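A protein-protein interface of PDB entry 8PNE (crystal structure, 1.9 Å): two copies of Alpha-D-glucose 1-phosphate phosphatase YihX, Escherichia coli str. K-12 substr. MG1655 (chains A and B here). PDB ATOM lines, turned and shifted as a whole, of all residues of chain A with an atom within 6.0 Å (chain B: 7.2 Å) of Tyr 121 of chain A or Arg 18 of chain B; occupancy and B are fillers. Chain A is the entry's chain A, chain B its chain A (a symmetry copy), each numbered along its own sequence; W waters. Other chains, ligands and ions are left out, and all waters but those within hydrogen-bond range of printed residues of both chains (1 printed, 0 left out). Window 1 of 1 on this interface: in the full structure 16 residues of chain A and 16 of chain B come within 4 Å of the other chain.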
ATOM      1  N   VAL A  12      -4.529 -29.831  13.179  1.00  0.00           N
ATOM      2  CA  VAL A  12      -4.953 -29.038  14.311  1.00  0.00           C
ATOM      3  C   VAL A  12      -5.818 -27.887  13.832  1.00  0.00           C
ATOM      4  O   VAL A  12      -5.576 -27.364  12.750  1.00  0.00           O
ATOM      5  CB  VAL A  12      -3.758 -28.489  15.097  1.00  0.00           C
ATOM      6  CG1 VAL A  12      -2.827 -29.593  15.599  1.00  0.00           C
ATOM      7  CG2 VAL A  12      -3.014 -27.436  14.288  1.00  0.00           C
ATOM      8  N   VAL A  81      -1.433 -18.720  21.080  1.00  0.00           N
ATOM      9  CA  VAL A  81      -2.215 -19.087  19.920  1.00  0.00           C
ATOM     10  C   VAL A  81      -3.071 -20.311  20.230  1.00  0.00           C
ATOM     11  O   VAL A  81      -2.604 -21.329  20.777  1.00  0.00           O
ATOM     12  CB  VAL A  81      -1.313 -19.326  18.689  1.00  0.00           C
ATOM     13  CG1 VAL A  81      -0.279 -20.411  18.917  1.00  0.00           C
ATOM     14  CG2 VAL A  81      -2.138 -19.668  17.473  1.00  0.00           C
ATOM     15  N   PHE A  82      -4.316 -20.253  19.759  1.00  0.00           N
ATOM     16  CA  PHE A  82      -5.234 -21.360  19.998  1.00  0.00           C
ATOM     17  C   PHE A  82      -4.847 -22.547  19.123  1.00  0.00           C
ATOM     18  O   PHE A  82      -4.783 -22.397  17.905  1.00  0.00           O
ATOM     19  CB  PHE A  82      -6.671 -20.938  19.710  1.00  0.00           C
ATOM     20  CG  PHE A  82      -7.664 -22.074  19.826  1.00  0.00           C
ATOM     21  CD1 PHE A  82      -8.039 -22.562  21.075  1.00  0.00           C
ATOM     22  CD2 PHE A  82      -8.183 -22.684  18.690  1.00  0.00           C
ATOM     23  CE1 PHE A  82      -8.908 -23.641  21.186  1.00  0.00           C
ATOM     24  CE2 PHE A  82      -9.072 -23.752  18.803  1.00  0.00           C
ATOM     25  CZ  PHE A  82      -9.431 -24.225  20.049  1.00  0.00           C
ATOM     26  N   VAL A  83      -4.615 -23.711  19.744  1.00  0.00           N
ATOM     27  CA  VAL A  83      -4.364 -24.944  19.015  1.00  0.00           C
ATOM     28  C   VAL A  83      -5.108 -26.121  19.654  1.00  0.00           C
ATOM     29  O   VAL A  83      -4.848 -26.500  20.790  1.00  0.00           O
ATOM     30  CB  VAL A  83      -2.861 -25.258  18.937  1.00  0.00           C
ATOM     31  CG1 VAL A  83      -2.632 -26.415  17.968  1.00  0.00           C
ATOM     32  CG2 VAL A  83      -2.007 -24.038  18.551  1.00  0.00           C
ATOM     33  N   ALA A  84      -5.979 -26.750  18.863  1.00  0.00           N
ATOM     34  CA  ALA A  84      -6.689 -27.964  19.236  1.00  0.00           C
ATOM     35  C   ALA A  84      -6.341 -29.081  18.252  1.00  0.00           C
ATOM     36  O   ALA A  84      -6.446 -28.877  17.053  1.00  0.00           O
ATOM     37  CB  ALA A  84      -8.180 -27.688  19.212  1.00  0.00           C
ATOM     38  N   LEU A  85      -5.980 -30.261  18.766  1.00  0.00           N
ATOM     39  CA  LEU A  85      -5.815 -31.440  17.940  1.00  0.00           C
ATOM     40  C   LEU A  85      -7.146 -31.839  17.302  1.00  0.00           C
ATOM     41  O   LEU A  85      -8.208 -31.584  17.856  1.00  0.00           O
ATOM     42  CB  LEU A  85      -5.285 -32.584  18.799  1.00  0.00           C
ATOM     43  CG  LEU A  85      -3.923 -32.362  19.432  1.00  0.00           C
ATOM     44  CD1 LEU A  85      -3.563 -33.516  20.356  1.00  0.00           C
ATOM     45  CD2 LEU A  85      -2.868 -32.183  18.356  1.00  0.00           C
ATOM     46  N   PHE A 116       6.497 -22.872  22.447  1.00  0.00           N
ATOM     47  CA  PHE A 116       6.089 -24.262  22.324  1.00  0.00           C
ATOM     48  C   PHE A 116       5.007 -24.344  21.254  1.00  0.00           C
ATOM     49  O   PHE A 116       3.915 -23.788  21.438  1.00  0.00           O
ATOM     50  CB  PHE A 116       5.590 -24.785  23.681  1.00  0.00           C
ATOM     51  CG  PHE A 116       5.108 -26.212  23.715  1.00  0.00           C
ATOM     52  CD1 PHE A 116       5.881 -27.240  23.205  1.00  0.00           C
ATOM     53  CD2 PHE A 116       3.911 -26.542  24.339  1.00  0.00           C
ATOM     54  CE1 PHE A 116       5.451 -28.555  23.257  1.00  0.00           C
ATOM     55  CE2 PHE A 116       3.464 -27.859  24.388  1.00  0.00           C
ATOM     56  CZ  PHE A 116       4.259 -28.867  23.878  1.00  0.00           C
ATOM     57  N   TRP A 117       5.317 -25.080  20.169  1.00  0.00           N
ATOM     58  CA  TRP A 117       4.536 -25.021  18.959  1.00  0.00           C
ATOM     59  C   TRP A 117       4.000 -26.405  18.621  1.00  0.00           C
ATOM     60  O   TRP A 117       4.552 -27.424  19.035  1.00  0.00           O
ATOM     61  CB  TRP A 117       5.419 -24.451  17.832  1.00  0.00           C
ATOM     62  CG  TRP A 117       4.810 -23.318  17.047  1.00  0.00           C
ATOM     63  CD1 TRP A 117       4.661 -23.274  15.695  1.00  0.00           C
ATOM     64  CD2 TRP A 117       4.252 -22.082  17.542  1.00  0.00           C
ATOM     65  NE1 TRP A 117       4.032 -22.131  15.313  1.00  0.00           N
ATOM     66  CE2 TRP A 117       3.801 -21.358  16.413  1.00  0.00           C
ATOM     67  CE3 TRP A 117       4.104 -21.503  18.810  1.00  0.00           C
ATOM     68  CZ2 TRP A 117       3.185 -20.109  16.515  1.00  0.00           C
ATOM     69  CZ3 TRP A 117       3.508 -20.257  18.906  1.00  0.00           C
ATOM     70  CH2 TRP A 117       3.023 -19.583  17.780  1.00  0.00           C
ATOM     71  N   PRO A 118       2.921 -26.496  17.810  1.00  0.00           N
ATOM     72  CA  PRO A 118       2.304 -27.787  17.490  1.00  0.00           C
ATOM     73  C   PRO A 118       3.284 -28.856  17.000  1.00  0.00           C
ATOM     74  O   PRO A 118       3.163 -30.028  17.372  1.00  0.00           O
ATOM     75  CB  PRO A 118       1.288 -27.455  16.372  1.00  0.00           C
ATOM     76  CG  PRO A 118       0.980 -25.984  16.556  1.00  0.00           C
ATOM     77  CD  PRO A 118       2.212 -25.362  17.188  1.00  0.00           C
ATOM     78  N   GLU A 119       4.282 -28.457  16.200  1.00  0.00           N
ATOM     79  CA  GLU A 119       5.195 -29.445  15.653  1.00  0.00           C
ATOM     80  C   GLU A 119       5.983 -30.059  16.798  1.00  0.00           C
ATOM     81  O   GLU A 119       6.460 -31.175  16.647  1.00  0.00           O
ATOM     82  CB  GLU A 119       6.123 -28.948  14.536  1.00  0.00           C
ATOM     83  CG  GLU A 119       7.051 -27.825  14.929  1.00  0.00           C
ATOM     84  CD  GLU A 119       6.447 -26.478  14.570  1.00  0.00           C
ATOM     85  OE1 GLU A 119       5.195 -26.417  14.398  1.00  0.00           O
ATOM     86  OE2 GLU A 119       7.230 -25.526  14.404  1.00  0.00           O
ATOM     87  N   GLU A 120       6.015 -29.389  17.956  1.00  0.00           N
ATOM     88  CA  GLU A 120       6.721 -29.928  19.116  1.00  0.00           C
ATOM     89  C   GLU A 120       5.781 -30.782  19.969  1.00  0.00           C
ATOM     90  O   GLU A 120       6.196 -31.373  20.921  1.00  0.00           O
ATOM     91  CB  GLU A 120       7.337 -28.793  19.940  1.00  0.00           C
ATOM     92  CG  GLU A 120       8.219 -27.872  19.122  1.00  0.00           C
ATOM     93  CD  GLU A 120       8.890 -26.758  19.921  1.00  0.00           C
ATOM     94  OE1 GLU A 120       8.186 -26.020  20.651  1.00  0.00           O
ATOM     95  OE2 GLU A 120      10.097 -26.674  19.861  1.00  0.00           O
ATOM     96  N   TYR A 121       4.509 -30.916  19.618  1.00  0.00           N
ATOM     97  CA  TYR A 121       3.607 -31.648  20.491  1.00  0.00           C
ATOM     98  C   TYR A 121       3.867 -33.150  20.358  1.00  0.00           C
ATOM     99  O   TYR A 121       3.833 -33.697  19.250  1.00  0.00           O
ATOM    100  CB  TYR A 121       2.141 -31.389  20.170  1.00  0.00           C
ATOM    101  CG  TYR A 121       1.572 -29.998  20.395  1.00  0.00           C
ATOM    102  CD1 TYR A 121       2.328 -28.927  20.875  1.00  0.00           C
ATOM    103  CD2 TYR A 121       0.263 -29.739  20.050  1.00  0.00           C
ATOM    104  CE1 TYR A 121       1.765 -27.671  21.055  1.00  0.00           C
ATOM    105  CE2 TYR A 121      -0.314 -28.488  20.233  1.00  0.00           C
ATOM    106  CZ  TYR A 121       0.437 -27.444  20.742  1.00  0.00           C
ATOM    107  OH  TYR A 121      -0.170 -26.222  20.854  1.00  0.00           O
ATOM    108  N   PRO A 122       4.042 -33.895  21.476  1.00  0.00           N
ATOM    109  CA  PRO A 122       4.323 -35.332  21.406  1.00  0.00           C
ATOM    110  C   PRO A 122       3.315 -36.123  20.583  1.00  0.00           C
ATOM    111  O   PRO A 122       3.694 -37.050  19.890  1.00  0.00           O
ATOM    112  CB  PRO A 122       4.276 -35.784  22.871  1.00  0.00           C
ATOM    113  CG  PRO A 122       4.620 -34.554  23.654  1.00  0.00           C
ATOM    114  CD  PRO A 122       4.022 -33.410  22.863  1.00  0.00           C
ATOM    115  N   GLU A 123       2.045 -35.716  20.621  1.00  0.00           N
ATOM    116  CA  GLU A 123       0.975 -36.440  19.958  1.00  0.00           C
ATOM    117  C   GLU A 123       1.103 -36.303  18.441  1.00  0.00           C
ATOM    118  O   GLU A 123       0.623 -37.154  17.684  1.00  0.00           O
ATOM    119  CB  GLU A 123      -0.396 -35.922  20.402  1.00  0.00           C
ATOM    120  CG  GLU A 123      -0.687 -36.054  21.901  1.00  0.00           C
ATOM    121  CD  GLU A 123      -0.116 -34.994  22.844  1.00  0.00           C
ATOM    122  OE1 GLU A 123       0.603 -34.047  22.395  1.00  0.00           O
ATOM    123  OE2 GLU A 123      -0.373 -35.121  24.054  1.00  0.00           O
ATOM    124  N   ILE A 124       1.720 -35.214  17.984  1.00  0.00           N
ATOM    125  CA  ILE A 124       1.827 -34.979  16.557  1.00  0.00           C
ATOM    126  C   ILE A 124       3.108 -35.632  16.063  1.00  0.00           C
ATOM    127  O   ILE A 124       3.081 -36.293  15.030  1.00  0.00           O
ATOM    128  CB  ILE A 124       1.716 -33.484  16.215  1.00  0.00           C
ATOM    129  CG1 ILE A 124       0.297 -32.988  16.515  1.00  0.00           C
ATOM    130  CG2 ILE A 124       2.088 -33.233  14.769  1.00  0.00           C
ATOM    131  CD1 ILE A 124       0.122 -31.496  16.408  1.00  0.00           C
ATOM    132  N   ARG A 125       4.197 -35.498  16.823  1.00  0.00           N
ATOM    133  CA  ARG A 125       5.412 -36.203  16.480  1.00  0.00           C
ATOM    134  C   ARG A 125       5.205 -37.720  16.427  1.00  0.00           C
ATOM    135  O   ARG A 125       5.677 -38.352  15.470  1.00  0.00           O
ATOM    136  CB  ARG A 125       6.524 -35.903  17.463  1.00  0.00           C
ATOM    137  CG  ARG A 125       6.960 -34.448  17.439  1.00  0.00           C
ATOM    138  CD  ARG A 125       8.030 -34.295  18.489  1.00  0.00           C
ATOM    139  NE  ARG A 125       8.855 -33.122  18.296  1.00  0.00           N
ATOM    140  CZ  ARG A 125       9.574 -32.558  19.269  1.00  0.00           C
ATOM    141  NH1 ARG A 125       9.500 -33.044  20.502  1.00  0.00           N
ATOM    142  NH2 ARG A 125      10.337 -31.502  19.014  1.00  0.00           N
ATOM    143  N   ASP A 126       4.507 -38.284  17.436  1.00  0.00           N
ATOM    144  CA  ASP A 126       4.320 -39.726  17.546  1.00  0.00           C
ATOM    145  C   ASP A 126       3.360 -40.214  16.450  1.00  0.00           C
ATOM    146  O   ASP A 126       3.253 -41.403  16.199  1.00  0.00           O
ATOM    147  CB  ASP A 126       3.889 -40.099  18.975  1.00  0.00           C
ATOM    148  CG  ASP A 126       4.958 -39.791  20.015  1.00  0.00           C
ATOM    149  OD1 ASP A 126       6.102 -39.550  19.621  1.00  0.00           O
ATOM    150  OD2 ASP A 126       4.639 -39.743  21.201  1.00  0.00           O
ATOM    151  N   ASP B  15      -7.069 -27.026  29.740  1.00  0.00           N
ATOM    152  CA  ASP B  15      -6.125 -28.099  29.939  1.00  0.00           C
ATOM    153  C   ASP B  15      -4.753 -27.533  30.250  1.00  0.00           C
ATOM    154  O   ASP B  15      -4.060 -27.093  29.339  1.00  0.00           O
ATOM    155  CB  ASP B  15      -6.070 -29.005  28.710  1.00  0.00           C
ATOM    156  CG  ASP B  15      -5.315 -30.293  28.988  1.00  0.00           C
ATOM    157  OD1 ASP B  15      -4.559 -30.348  30.011  1.00  0.00           O
ATOM    158  OD2 ASP B  15      -5.502 -31.231  28.197  1.00  0.00           O
ATOM    159  N   PHE B  16      -4.348 -27.669  31.517  1.00  0.00           N
ATOM    160  CA  PHE B  16      -3.054 -27.198  31.977  1.00  0.00           C
ATOM    161  C   PHE B  16      -1.910 -28.136  31.592  1.00  0.00           C
ATOM    162  O   PHE B  16      -0.748 -27.774  31.822  1.00  0.00           O
ATOM    163  CB  PHE B  16      -3.058 -26.941  33.486  1.00  0.00           C
ATOM    164  CG  PHE B  16      -3.709 -25.639  33.867  1.00  0.00           C
ATOM    165  CD1 PHE B  16      -5.090 -25.514  33.963  1.00  0.00           C
ATOM    166  CD2 PHE B  16      -2.931 -24.515  34.089  1.00  0.00           C
ATOM    167  CE1 PHE B  16      -5.680 -24.304  34.317  1.00  0.00           C
ATOM    168  CE2 PHE B  16      -3.521 -23.293  34.395  1.00  0.00           C
ATOM    169  CZ  PHE B  16      -4.889 -23.181  34.493  1.00  0.00           C
ATOM    170  N   ASN B  17      -2.189 -29.284  30.961  1.00  0.00           N
ATOM    171  CA  ASN B  17      -1.084 -30.095  30.431  1.00  0.00           C
ATOM    172  C   ASN B  17      -0.309 -29.380  29.314  1.00  0.00           C
ATOM    173  O   ASN B  17       0.894 -29.571  29.147  1.00  0.00           O
ATOM    174  CB  ASN B  17      -1.545 -31.448  29.905  1.00  0.00           C
ATOM    175  CG  ASN B  17      -1.853 -32.407  31.031  1.00  0.00           C
ATOM    176  OD1 ASN B  17      -1.126 -32.470  32.018  1.00  0.00           O
ATOM    177  ND2 ASN B  17      -2.938 -33.147  30.883  1.00  0.00           N
ATOM    178  N   ARG B  18      -0.994 -28.521  28.566  1.00  0.00           N
ATOM    179  CA  ARG B  18      -0.336 -27.655  27.611  1.00  0.00           C
ATOM    180  C   ARG B  18       0.758 -26.803  28.273  1.00  0.00           C
ATOM    181  O   ARG B  18       1.823 -26.616  27.694  1.00  0.00           O
ATOM    182  CB  ARG B  18      -1.426 -26.838  26.906  1.00  0.00           C
ATOM    183  CG  ARG B  18      -0.961 -26.209  25.610  1.00  0.00           C
ATOM    184  CD  ARG B  18      -0.659 -27.134  24.458  1.00  0.00           C
ATOM    185  NE  ARG B  18      -1.815 -27.865  23.912  1.00  0.00           N
ATOM    186  CZ  ARG B  18      -2.693 -27.430  23.018  1.00  0.00           C
ATOM    187  NH1 ARG B  18      -2.793 -26.152  22.693  1.00  0.00           N
ATOM    188  NH2 ARG B  18      -3.549 -28.297  22.505  1.00  0.00           N
ATOM    189  N   VAL B  19       0.495 -26.293  29.478  1.00  0.00           N
ATOM    190  CA  VAL B  19       1.446 -25.469  30.217  1.00  0.00           C
ATOM    191  C   VAL B  19       2.662 -26.325  30.583  1.00  0.00           C
ATOM    192  O   VAL B  19       3.804 -25.906  30.463  1.00  0.00           O
ATOM    193  CB  VAL B  19       0.813 -24.866  31.493  1.00  0.00           C
ATOM    194  CG1 VAL B  19       1.820 -24.062  32.285  1.00  0.00           C
ATOM    195  CG2 VAL B  19      -0.397 -23.985  31.209  1.00  0.00           C
ATOM    196  N   LEU B  20       2.410 -27.551  31.031  1.00  0.00           N
ATOM    197  CA  LEU B  20       3.486 -28.448  31.446  1.00  0.00           C
ATOM    198  C   LEU B  20       4.344 -28.750  30.223  1.00  0.00           C
ATOM    199  O   LEU B  20       5.565 -28.645  30.304  1.00  0.00           O
ATOM    200  CB  LEU B  20       2.899 -29.722  32.082  1.00  0.00           C
ATOM    201  CG  LEU B  20       2.023 -29.484  33.328  1.00  0.00           C
ATOM    202  CD1 LEU B  20       1.626 -30.771  33.999  1.00  0.00           C
ATOM    203  CD2 LEU B  20       2.717 -28.593  34.339  1.00  0.00           C
ATOM    204  N   GLY B  21       3.671 -28.979  29.079  1.00  0.00           N
ATOM    205  CA  GLY B  21       4.345 -29.140  27.803  1.00  0.00           C
ATOM    206  C   GLY B  21       5.254 -27.958  27.478  1.00  0.00           C
ATOM    207  O   GLY B  21       6.378 -28.139  27.033  1.00  0.00           O
ATOM    208  N   ALA B  22       4.772 -26.742  27.743  1.00  0.00           N
ATOM    209  CA  ALA B  22       5.537 -25.568  27.395  1.00  0.00           C
ATOM    210  C   ALA B  22       6.727 -25.419  28.334  1.00  0.00           C
ATOM    211  O   ALA B  22       7.828 -25.046  27.925  1.00  0.00           O
ATOM    212  CB  ALA B  22       4.632 -24.371  27.443  1.00  0.00           C
ATOM    213  N   TRP B  23       6.515 -25.691  29.617  1.00  0.00           N
ATOM    214  CA  TRP B  23       7.630 -25.637  30.553  1.00  0.00           C
ATOM    215  C   TRP B  23       8.648 -26.745  30.271  1.00  0.00           C
ATOM    216  O   TRP B  23       9.849 -26.542  30.473  1.00  0.00           O
ATOM    217  CB  TRP B  23       7.120 -25.743  31.991  1.00  0.00           C
ATOM    218  CG  TRP B  23       6.454 -24.518  32.534  1.00  0.00           C
ATOM    219  CD1 TRP B  23       6.628 -23.227  32.122  1.00  0.00           C
ATOM    220  CD2 TRP B  23       5.480 -24.486  33.596  1.00  0.00           C
ATOM    221  NE1 TRP B  23       5.882 -22.394  32.901  1.00  0.00           N
ATOM    222  CE2 TRP B  23       5.138 -23.128  33.790  1.00  0.00           C
ATOM    223  CE3 TRP B  23       4.860 -25.455  34.393  1.00  0.00           C
ATOM    224  CZ2 TRP B  23       4.205 -22.723  34.740  1.00  0.00           C
ATOM    225  CZ3 TRP B  23       3.973 -25.046  35.363  1.00  0.00           C
ATOM    226  CH2 TRP B  23       3.620 -23.702  35.504  1.00  0.00           C
ATOM    227  N   SER B  24       8.160 -27.910  29.821  1.00  0.00           N
ATOM    228  CA  SER B  24       9.040 -29.003  29.430  1.00  0.00           C
ATOM    229  C   SER B  24       9.861 -28.586  28.219  1.00  0.00           C
ATOM    230  O   SER B  24      11.072 -28.850  28.156  1.00  0.00           O
ATOM    231  CB  SER B  24       8.267 -30.284  29.168  1.00  0.00           C
ATOM    232  OG  SER B  24       9.112 -31.362  28.763  1.00  0.00           O
ATOM    233  N   LEU B  31       8.298 -34.363  30.634  1.00  0.00           N
ATOM    234  CA  LEU B  31       6.931 -34.007  30.925  1.00  0.00           C
ATOM    235  C   LEU B  31       6.442 -34.794  32.138  1.00  0.00           C
ATOM    236  O   LEU B  31       5.704 -34.239  32.962  1.00  0.00           O
ATOM    237  CB  LEU B  31       6.078 -34.282  29.690  1.00  0.00           C
ATOM    238  CG  LEU B  31       4.594 -34.005  29.854  1.00  0.00           C
ATOM    239  CD1 LEU B  31       4.358 -32.540  30.188  1.00  0.00           C
ATOM    240  CD2 LEU B  31       3.843 -34.418  28.596  1.00  0.00           C
ATOM    241  N   LYS B  35       4.249 -33.596  35.332  1.00  0.00           N
ATOM    242  CA  LYS B  35       2.929 -34.110  35.655  1.00  0.00           C
ATOM    243  C   LYS B  35       2.884 -34.645  37.085  1.00  0.00           C
ATOM    244  O   LYS B  35       1.875 -34.482  37.748  1.00  0.00           O
ATOM    245  CB  LYS B  35       2.463 -35.200  34.681  1.00  0.00           C
ATOM    246  CG  LYS B  35       1.895 -34.623  33.398  1.00  0.00           C
ATOM    247  CD  LYS B  35       1.439 -35.624  32.375  1.00  0.00           C
ATOM    248  CE  LYS B  35       1.068 -34.895  31.106  1.00  0.00           C
ATOM    249  NZ  LYS B  35       0.316 -35.760  30.162  1.00  0.00           N
ATOM    250  N   GLY B  77       4.996 -19.711  29.855  1.00  0.00           N
ATOM    251  CA  GLY B  77       4.340 -21.007  29.714  1.00  0.00           C
ATOM    252  C   GLY B  77       2.885 -21.068  30.205  1.00  0.00           C
ATOM    253  O   GLY B  77       2.048 -21.840  29.680  1.00  0.00           O
ATOM    254  N   TRP B  78       2.624 -20.410  31.334  1.00  0.00           N
ATOM    255  CA  TRP B  78       1.273 -20.309  31.893  1.00  0.00           C
ATOM    256  C   TRP B  78       0.323 -19.816  30.816  1.00  0.00           C
ATOM    257  O   TRP B  78      -0.802 -20.333  30.660  1.00  0.00           O
ATOM    258  CB  TRP B  78       1.309 -19.376  33.121  1.00  0.00           C
ATOM    259  CG  TRP B  78       0.195 -19.510  34.122  1.00  0.00           C
ATOM    260  CD1 TRP B  78      -0.725 -18.568  34.496  1.00  0.00           C
ATOM    261  CD2 TRP B  78      -0.056 -20.657  34.942  1.00  0.00           C
ATOM    262  NE1 TRP B  78      -1.586 -19.072  35.435  1.00  0.00           N
ATOM    263  CE2 TRP B  78      -1.174 -20.339  35.756  1.00  0.00           C
ATOM    264  CE3 TRP B  78       0.568 -21.905  35.075  1.00  0.00           C
ATOM    265  CZ2 TRP B  78      -1.684 -21.246  36.678  1.00  0.00           C
ATOM    266  CZ3 TRP B  78       0.067 -22.783  35.998  1.00  0.00           C
ATOM    267  CH2 TRP B  78      -1.035 -22.455  36.800  1.00  0.00           C
ATOM    268  N   ALA B  80       0.220 -20.557  27.953  1.00  0.00           N
ATOM    269  CA  ALA B  80       0.021 -21.491  26.859  1.00  0.00           C
ATOM    270  C   ALA B  80      -1.207 -22.354  27.100  1.00  0.00           C
ATOM    271  O   ALA B  80      -1.496 -23.192  26.267  1.00  0.00           O
ATOM    272  CB  ALA B  80       1.217 -22.355  26.655  1.00  0.00           C
ATOM    273  N   VAL B  81      -1.881 -22.161  28.229  1.00  0.00           N
ATOM    274  CA  VAL B  81      -2.904 -23.094  28.651  1.00  0.00           C
ATOM    275  C   VAL B  81      -3.959 -23.245  27.559  1.00  0.00           C
ATOM    276  O   VAL B  81      -4.475 -22.263  26.992  1.00  0.00           O
ATOM    277  CB  VAL B  81      -3.538 -22.661  29.992  1.00  0.00           C
ATOM    278  CG1 VAL B  81      -4.160 -21.280  29.932  1.00  0.00           C
ATOM    279  CG2 VAL B  81      -4.573 -23.659  30.446  1.00  0.00           C
ATOM    280  N   PHE B  82      -4.370 -24.495  27.352  1.00  0.00           N
ATOM    281  CA  PHE B  82      -5.370 -24.769  26.328  1.00  0.00           C
ATOM    282  C   PHE B  82      -6.737 -24.287  26.802  1.00  0.00           C
ATOM    283  O   PHE B  82      -7.188 -24.716  27.862  1.00  0.00           O
ATOM    284  CB  PHE B  82      -5.417 -26.260  26.008  1.00  0.00           C
ATOM    285  CG  PHE B  82      -6.516 -26.630  25.036  1.00  0.00           C
ATOM    286  CD1 PHE B  82      -6.397 -26.326  23.683  1.00  0.00           C
ATOM    287  CD2 PHE B  82      -7.685 -27.236  25.481  1.00  0.00           C
ATOM    288  CE1 PHE B  82      -7.426 -26.613  22.795  1.00  0.00           C
ATOM    289  CE2 PHE B  82      -8.708 -27.544  24.586  1.00  0.00           C
ATOM    290  CZ  PHE B  82      -8.574 -27.233  23.248  1.00  0.00           C
ATOM    291  N   VAL B  83      -7.386 -23.424  26.011  1.00  0.00           N
ATOM    292  CA  VAL B  83      -8.746 -22.990  26.286  1.00  0.00           C
ATOM    293  C   VAL B  83      -9.579 -22.948  25.001  1.00  0.00           C
ATOM    294  O   VAL B  83      -9.303 -22.183  24.084  1.00  0.00           O
ATOM    295  CB  VAL B  83      -8.772 -21.612  26.968  1.00  0.00           C
ATOM    296  CG1 VAL B  83     -10.188 -21.310  27.451  1.00  0.00           C
ATOM    297  CG2 VAL B  83      -7.758 -21.488  28.118  1.00  0.00           C
HETATM  298  O   HOH W   1      -3.942 -23.456  22.634  1.00  0.00           O
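Of the 17 printed residues of chain A, 5 touch a printed residue of chain B.
Water W1 lies within hydrogen-bond range of NH1 of Arg 18 of chain B (2.9 Å), N of Val 83 of chain A (3.0 Å) and O of Val 81 of chain A (3.1 Å).
Among the printed residues, pairs that only touch across the chains: Val 83 of chain A with Phe 82 of chain B (3.3 Å), Phe 82 of chain A with Val 83 of chain B (3.3 Å), Phe 116 of chain A with Ala 22 of chain B (3.5 Å), Phe 116 of chain A with Gly 21 of chain B (3.6 Å), Phe 82 of chain A with Phe 82 of chain B (3.7 Å), Ala 84 of chain A with Phe 82 of chain B (3.8 Å) and Phe 116 of chain A with Arg 18 of chain B (3.9 Å).
The backbone carbonyl oxygen (O) of Val 83 of chain A sits at hydrogen-bond distance from the guanidinium group (NH2) of Arg 18 of chain B (2.8 Å). The guanidinium group of Arg 18 of chain B sits at hydrogen-bond distance from the side-chain hydroxyl of Tyr 121 of chain A (3.2 Å).
The backbone NH (N) of Asp 15 of chain B sits at hydrogen-bond distance from the backbone carbonyl oxygen (O) of Phe 82 of chain B, at 3.0 Å.
Val 81 of chain A touches none of the printed residues of chain B. Of the printed residues of chain B, Val 83 of chain A touches Arg 18 and Phe 82. Of the printed residues of chain B, Phe 116 of chain A touches Arg 18, Gly 21 and Ala 22. Tyr 121 of chain A touches one residue of chain B. Of chain A, only Val 83 (2.8 Å), Phe 116 (3.9 Å) and Tyr 121 (3.2 Å) come within 4 Å of Arg 18 of chain B. Val 19 of chain B touches none of the printed residues of chain A. Of the printed residues of chain A, Ala 22 of chain B touches Phe 116. The nearest residue of chain A that does not touch Arg 18 of chain B is Ala 84 of chain A (4.5 Å). The nearest printed residue of chain A that does not touch Gly 21 of chain B is Pro 122 of chain A (6.5 Å).
Phe 82 of chain B touches its own counterpart, Phe 82 of chain A. Phe 82 of chain A touches Val 83 of chain B, and with the chains exchanged Val 83 of chain A touches Phe 82 of chain B. Of the 9 pairs that touch across the chains among the printed residues, 3 have their exchanged pair printed and touching as well.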
